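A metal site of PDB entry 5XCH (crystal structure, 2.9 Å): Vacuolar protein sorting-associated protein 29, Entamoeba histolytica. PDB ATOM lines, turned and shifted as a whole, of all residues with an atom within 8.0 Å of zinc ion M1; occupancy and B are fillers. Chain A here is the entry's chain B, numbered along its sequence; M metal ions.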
ATOM      1  N   ASP A   8      15.644  23.533  -0.778  1.00  0.00           N
ATOM      2  CA  ASP A   8      16.148  24.669  -1.566  1.00  0.00           C
ATOM      3  C   ASP A   8      15.116  25.785  -1.661  1.00  0.00           C
ATOM      4  O   ASP A   8      14.757  26.244  -2.756  1.00  0.00           O
ATOM      5  CB  ASP A   8      16.603  24.200  -2.945  1.00  0.00           C
ATOM      6  CG  ASP A   8      17.874  23.377  -2.899  1.00  0.00           C
ATOM      7  OD1 ASP A   8      18.963  23.972  -3.009  1.00  0.00           O
ATOM      8  OD2 ASP A   8      17.769  22.146  -2.733  1.00  0.00           O
ATOM      9  N   PHE A   9      14.648  26.245  -0.504  1.00  0.00           N
ATOM     10  CA  PHE A   9      13.510  27.160  -0.450  1.00  0.00           C
ATOM     11  C   PHE A   9      13.874  28.628  -0.586  1.00  0.00           C
ATOM     12  O   PHE A   9      12.987  29.438  -0.826  1.00  0.00           O
ATOM     13  CB  PHE A   9      12.743  26.968   0.861  1.00  0.00           C
ATOM     14  CG  PHE A   9      12.234  25.573   1.067  1.00  0.00           C
ATOM     15  CD1 PHE A   9      11.096  25.122   0.416  1.00  0.00           C
ATOM     16  CD2 PHE A   9      12.875  24.711   1.931  1.00  0.00           C
ATOM     17  CE1 PHE A   9      10.626  23.847   0.609  1.00  0.00           C
ATOM     18  CE2 PHE A   9      12.414  23.431   2.134  1.00  0.00           C
ATOM     19  CZ  PHE A   9      11.288  22.996   1.478  1.00  0.00           C
ATOM     20  N   HIS A  10      15.148  29.008  -0.423  1.00  0.00           N
ATOM     21  CA  HIS A  10      15.424  30.434  -0.378  1.00  0.00           C
ATOM     22  C   HIS A  10      16.872  30.730  -0.735  1.00  0.00           C
ATOM     23  O   HIS A  10      17.737  29.863  -0.729  1.00  0.00           O
ATOM     24  CB  HIS A  10      15.080  31.021   0.988  1.00  0.00           C
ATOM     25  CG  HIS A  10      14.449  32.381   0.912  1.00  0.00           C
ATOM     26  ND1 HIS A  10      14.178  33.144   2.036  1.00  0.00           N
ATOM     27  CD2 HIS A  10      14.028  33.109  -0.145  1.00  0.00           C
ATOM     28  CE1 HIS A  10      13.621  34.274   1.670  1.00  0.00           C
ATOM     29  NE2 HIS A  10      13.510  34.283   0.356  1.00  0.00           N
ATOM     30  N   THR A  37      16.635  18.585   1.434  1.00  0.00           N
ATOM     31  CA  THR A  37      18.025  18.819   1.063  1.00  0.00           C
ATOM     32  C   THR A  37      18.609  20.036   1.752  1.00  0.00           C
ATOM     33  O   THR A  37      19.836  20.205   1.751  1.00  0.00           O
ATOM     34  CB  THR A  37      18.170  18.981  -0.454  1.00  0.00           C
ATOM     35  OG1 THR A  37      17.556  20.204  -0.867  1.00  0.00           O
ATOM     36  CG2 THR A  37      17.514  17.819  -1.182  1.00  0.00           C
ATOM     37  N   GLY A  38      17.768  20.884   2.338  1.00  0.00           N
ATOM     38  CA  GLY A  38      18.206  22.070   3.032  1.00  0.00           C
ATOM     39  C   GLY A  38      17.795  23.343   2.306  1.00  0.00           C
ATOM     40  O   GLY A  38      16.873  23.362   1.491  1.00  0.00           O
ATOM     41  N   ASN A  39      18.513  24.417   2.622  1.00  0.00           N
ATOM     42  CA  ASN A  39      18.260  25.747   2.070  1.00  0.00           C
ATOM     43  C   ASN A  39      16.809  26.179   2.305  1.00  0.00           C
ATOM     44  O   ASN A  39      16.090  26.580   1.391  1.00  0.00           O
ATOM     45  CB  ASN A  39      18.627  25.805   0.581  1.00  0.00           C
ATOM     46  CG  ASN A  39      19.707  26.816   0.294  1.00  0.00           C
ATOM     47  OD1 ASN A  39      19.711  27.464  -0.758  1.00  0.00           O
ATOM     48  ND2 ASN A  39      20.637  26.972   1.225  1.00  0.00           N
ATOM     49  N   LYS A  60      22.634  20.768   5.813  1.00  0.00           N
ATOM     50  CA  LYS A  60      23.226  22.105   5.717  1.00  0.00           C
ATOM     51  C   LYS A  60      23.488  22.491   4.272  1.00  0.00           C
ATOM     52  O   LYS A  60      23.860  21.655   3.442  1.00  0.00           O
ATOM     53  CB  LYS A  60      24.571  22.194   6.427  1.00  0.00           C
ATOM     54  CG  LYS A  60      24.497  22.231   7.933  1.00  0.00           C
ATOM     55  CD  LYS A  60      25.444  21.069   8.495  1.00  0.00           C
ATOM     56  CE  LYS A  60      25.211  20.722   9.930  1.00  0.00           C
ATOM     57  NZ  LYS A  60      26.045  19.677  10.479  1.00  0.00           N
ATOM     58  N   GLY A  61      23.340  23.772   3.979  1.00  0.00           N
ATOM     59  CA  GLY A  61      23.645  24.298   2.660  1.00  0.00           C
ATOM     60  C   GLY A  61      24.241  25.686   2.718  1.00  0.00           C
ATOM     61  O   GLY A  61      24.955  26.039   3.658  1.00  0.00           O
ATOM     62  N   ASP A  62      23.924  26.472   1.689  1.00  0.00           N
ATOM     63  CA  ASP A  62      24.593  27.747   1.469  1.00  0.00           C
ATOM     64  C   ASP A  62      24.277  28.754   2.580  1.00  0.00           C
ATOM     65  O   ASP A  62      25.182  29.276   3.242  1.00  0.00           O
ATOM     66  CB  ASP A  62      24.191  28.308   0.108  1.00  0.00           C
ATOM     67  CG  ASP A  62      24.049  27.232  -0.950  1.00  0.00           C
ATOM     68  OD1 ASP A  62      24.877  26.298  -0.969  1.00  0.00           O
ATOM     69  OD2 ASP A  62      23.116  27.321  -1.765  1.00  0.00           O
ATOM     70  N   PHE A  63      22.991  29.023   2.797  1.00  0.00           N
ATOM     71  CA  PHE A  63      22.547  30.064   3.726  1.00  0.00           C
ATOM     72  C   PHE A  63      21.639  29.484   4.800  1.00  0.00           C
ATOM     73  O   PHE A  63      20.605  30.058   5.149  1.00  0.00           O
ATOM     74  CB  PHE A  63      21.830  31.189   2.985  1.00  0.00           C
ATOM     75  CG  PHE A  63      22.352  31.422   1.579  1.00  0.00           C
ATOM     76  CD1 PHE A  63      21.737  30.819   0.492  1.00  0.00           C
ATOM     77  CD2 PHE A  63      23.438  32.253   1.351  1.00  0.00           C
ATOM     78  CE1 PHE A  63      22.204  31.023  -0.789  1.00  0.00           C
ATOM     79  CE2 PHE A  63      23.910  32.465   0.068  1.00  0.00           C
ATOM     80  CZ  PHE A  63      23.286  31.848  -1.006  1.00  0.00           C
ATOM     81  N   ASP A  64      22.011  28.332   5.348  1.00  0.00           N
ATOM     82  CA  ASP A  64      21.265  27.685   6.420  1.00  0.00           C
ATOM     83  C   ASP A  64      21.967  27.943   7.744  1.00  0.00           C
ATOM     84  O   ASP A  64      23.190  27.849   7.836  1.00  0.00           O
ATOM     85  CB  ASP A  64      21.125  26.181   6.164  1.00  0.00           C
ATOM     86  CG  ASP A  64      20.938  25.853   4.699  1.00  0.00           C
ATOM     87  OD1 ASP A  64      21.482  26.589   3.845  1.00  0.00           O
ATOM     88  OD2 ASP A  64      20.261  24.853   4.397  1.00  0.00           O
ATOM     89  N   HIS A  86      23.244  17.994   0.413  1.00  0.00           N
ATOM     90  CA  HIS A  86      22.819  19.245  -0.194  1.00  0.00           C
ATOM     91  C   HIS A  86      23.410  19.470  -1.578  1.00  0.00           C
ATOM     92  O   HIS A  86      22.746  20.046  -2.445  1.00  0.00           O
ATOM     93  CB  HIS A  86      23.192  20.420   0.724  1.00  0.00           C
ATOM     94  CG  HIS A  86      22.678  21.748   0.261  1.00  0.00           C
ATOM     95  ND1 HIS A  86      21.344  22.107   0.347  1.00  0.00           N
ATOM     96  CD2 HIS A  86      23.317  22.808  -0.290  1.00  0.00           C
ATOM     97  CE1 HIS A  86      21.184  23.326  -0.128  1.00  0.00           C
ATOM     98  NE2 HIS A  86      22.373  23.777  -0.516  1.00  0.00           N
ATOM     99  N   GLY A  87      24.653  19.040  -1.804  1.00  0.00           N
ATOM    100  CA  GLY A  87      25.306  19.212  -3.075  1.00  0.00           C
ATOM    101  C   GLY A  87      26.341  20.321  -3.105  1.00  0.00           C
ATOM    102  O   GLY A  87      27.215  20.307  -3.979  1.00  0.00           O
ATOM    103  N   HIS A  88      26.273  21.266  -2.171  1.00  0.00           N
ATOM    104  CA  HIS A  88      27.269  22.338  -2.108  1.00  0.00           C
ATOM    105  C   HIS A  88      28.662  21.793  -1.816  1.00  0.00           C
ATOM    106  O   HIS A  88      29.654  22.495  -2.031  1.00  0.00           O
ATOM    107  CB  HIS A  88      26.874  23.373  -1.061  1.00  0.00           C
ATOM    108  CG  HIS A  88      27.595  23.234   0.240  1.00  0.00           C
ATOM    109  ND1 HIS A  88      28.788  23.890   0.515  1.00  0.00           N
ATOM    110  CD2 HIS A  88      27.300  22.524   1.362  1.00  0.00           C
ATOM    111  CE1 HIS A  88      29.187  23.584   1.734  1.00  0.00           C
ATOM    112  NE2 HIS A  88      28.308  22.757   2.270  1.00  0.00           N
ATOM    113  N   GLY A 114      20.668  18.611  -4.028  1.00  0.00           N
ATOM    114  CA  GLY A 114      20.107  19.934  -4.250  1.00  0.00           C
ATOM    115  C   GLY A 114      21.115  20.874  -4.863  1.00  0.00           C
ATOM    116  O   GLY A 114      22.099  20.424  -5.459  1.00  0.00           O
ATOM    117  N   HIS A 115      20.872  22.181  -4.738  1.00  0.00           N
ATOM    118  CA  HIS A 115      21.804  23.245  -5.084  1.00  0.00           C
ATOM    119  C   HIS A 115      21.854  23.546  -6.578  1.00  0.00           C
ATOM    120  O   HIS A 115      22.352  24.595  -6.984  1.00  0.00           O
ATOM    121  CB  HIS A 115      23.209  22.929  -4.553  1.00  0.00           C
ATOM    122  CG  HIS A 115      24.115  24.114  -4.506  1.00  0.00           C
ATOM    123  ND1 HIS A 115      23.806  25.263  -3.806  1.00  0.00           N
ATOM    124  CD2 HIS A 115      25.321  24.342  -5.075  1.00  0.00           C
ATOM    125  CE1 HIS A 115      24.777  26.137  -3.943  1.00  0.00           C
ATOM    126  NE2 HIS A 115      25.710  25.606  -4.703  1.00  0.00           N
ATOM    127  N   THR A 116      21.345  22.640  -7.418  1.00  0.00           N
ATOM    128  CA  THR A 116      21.113  22.993  -8.811  1.00  0.00           C
ATOM    129  C   THR A 116      19.790  23.714  -9.007  1.00  0.00           C
ATOM    130  O   THR A 116      19.621  24.429  -9.995  1.00  0.00           O
ATOM    131  CB  THR A 116      21.142  21.757  -9.714  1.00  0.00           C
ATOM    132  OG1 THR A 116      20.187  20.793  -9.237  1.00  0.00           O
ATOM    133  CG2 THR A 116      22.518  21.131  -9.734  1.00  0.00           C
ATOM    134  N   HIS A 117      18.850  23.553  -8.066  1.00  0.00           N
ATOM    135  CA  HIS A 117      17.531  24.173  -8.104  1.00  0.00           C
ATOM    136  C   HIS A 117      16.720  23.729  -9.323  1.00  0.00           C
ATOM    137  O   HIS A 117      15.873  24.468  -9.822  1.00  0.00           O
ATOM    138  CB  HIS A 117      17.638  25.707  -8.063  1.00  0.00           C
ATOM    139  CG  HIS A 117      17.965  26.246  -6.711  1.00  0.00           C
ATOM    140  ND1 HIS A 117      17.748  27.565  -6.367  1.00  0.00           N
ATOM    141  CD2 HIS A 117      18.481  25.647  -5.616  1.00  0.00           C
ATOM    142  CE1 HIS A 117      18.125  27.752  -5.110  1.00  0.00           C
ATOM    143  NE2 HIS A 117      18.571  26.604  -4.634  1.00  0.00           N
ATOM    144  N   SER A 140      19.183  30.257  -8.589  1.00  0.00           N
ATOM    145  CA  SER A 140      20.549  29.911  -8.284  1.00  0.00           C
ATOM    146  C   SER A 140      21.480  30.506  -9.332  1.00  0.00           C
ATOM    147  O   SER A 140      21.051  30.935 -10.403  1.00  0.00           O
ATOM    148  CB  SER A 140      20.728  28.393  -8.234  1.00  0.00           C
ATOM    149  OG  SER A 140      21.971  28.026  -7.673  1.00  0.00           O
ATOM    150  N   PRO A 141      22.759  30.567  -9.017  1.00  0.00           N
ATOM    151  CA  PRO A 141      23.788  30.785 -10.030  1.00  0.00           C
ATOM    152  C   PRO A 141      23.541  30.014 -11.326  1.00  0.00           C
ATOM    153  O   PRO A 141      23.866  30.509 -12.409  1.00  0.00           O
ATOM    154  CB  PRO A 141      25.061  30.268  -9.328  1.00  0.00           C
ATOM    155  CG  PRO A 141      24.770  30.465  -7.807  1.00  0.00           C
ATOM    156  CD  PRO A 141      23.304  30.761  -7.652  1.00  0.00           C
ATOM    157  N   LEU A 142      22.926  28.831 -11.230  1.00  0.00           N
ATOM    158  CA  LEU A 142      22.865  27.937 -12.379  1.00  0.00           C
ATOM    159  C   LEU A 142      21.673  28.252 -13.296  1.00  0.00           C
ATOM    160  O   LEU A 142      21.809  28.205 -14.523  1.00  0.00           O
ATOM    161  CB  LEU A 142      22.806  26.488 -11.899  1.00  0.00           C
ATOM    162  CG  LEU A 142      23.943  25.948 -11.031  1.00  0.00           C
ATOM    163  CD1 LEU A 142      25.305  26.452 -11.512  1.00  0.00           C
ATOM    164  CD2 LEU A 142      23.754  26.253  -9.541  1.00  0.00           C
HETATM  165 ZN    ZN M   1      22.204  25.600  -2.300  1.00  0.00          ZN
HETATM  166 ZN    ZN M   2      19.515  26.683  -2.784  1.00  0.00          ZN
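OD2 of Asp 62 binds zinc ion M1 (2.0 Å). Zinc ion M1 is bound by ND1 of His 115 (2.2 Å). NE2 of His 86 is bound to zinc ion M1 (2.6 Å). Zinc ion M1 has three donor atoms within binding distance.
Residues that only touch zinc ion M1: Asp 8 (3.7 Å) and Asn 39 (3.5 Å). Five residues have an atom within 4 Å of zinc ion M1: Asp 8, Asn 39, Asp 62, His 86 and His 115.
The side-chain hydroxyl of Thr 37 is in hydrogen-bond range of the side-chain carboxylate of Asp 8. N of Asn 39 sits at hydrogen-bond distance from OD2 of Asp 64 (2.5 Å). The side-chain carboxylate (OD1) of Asp 8 sits close to a ring nitrogen (NE2) of His 117, at 3.1 Å. A ring nitrogen (ND1) of His 86 sits at hydrogen-bond distance from the backbone carbonyl oxygen (O) of Thr 37, 2.8 Å away. ND2 of Asn 39 sits close to N of Asp 62 (3.4 Å). The backbone carbonyl oxygen (O) of Asn 39 lies within hydrogen-bond range of the backbone NH (N) of His 10, at 3.2 Å. OD1 of Asp 64 is in hydrogen-bond range of N of Asp 62 (3.3 Å). The backbone NH of His 115 is in hydrogen-bond range of the side-chain carboxylate of Asp 8, 3.1 Å away.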
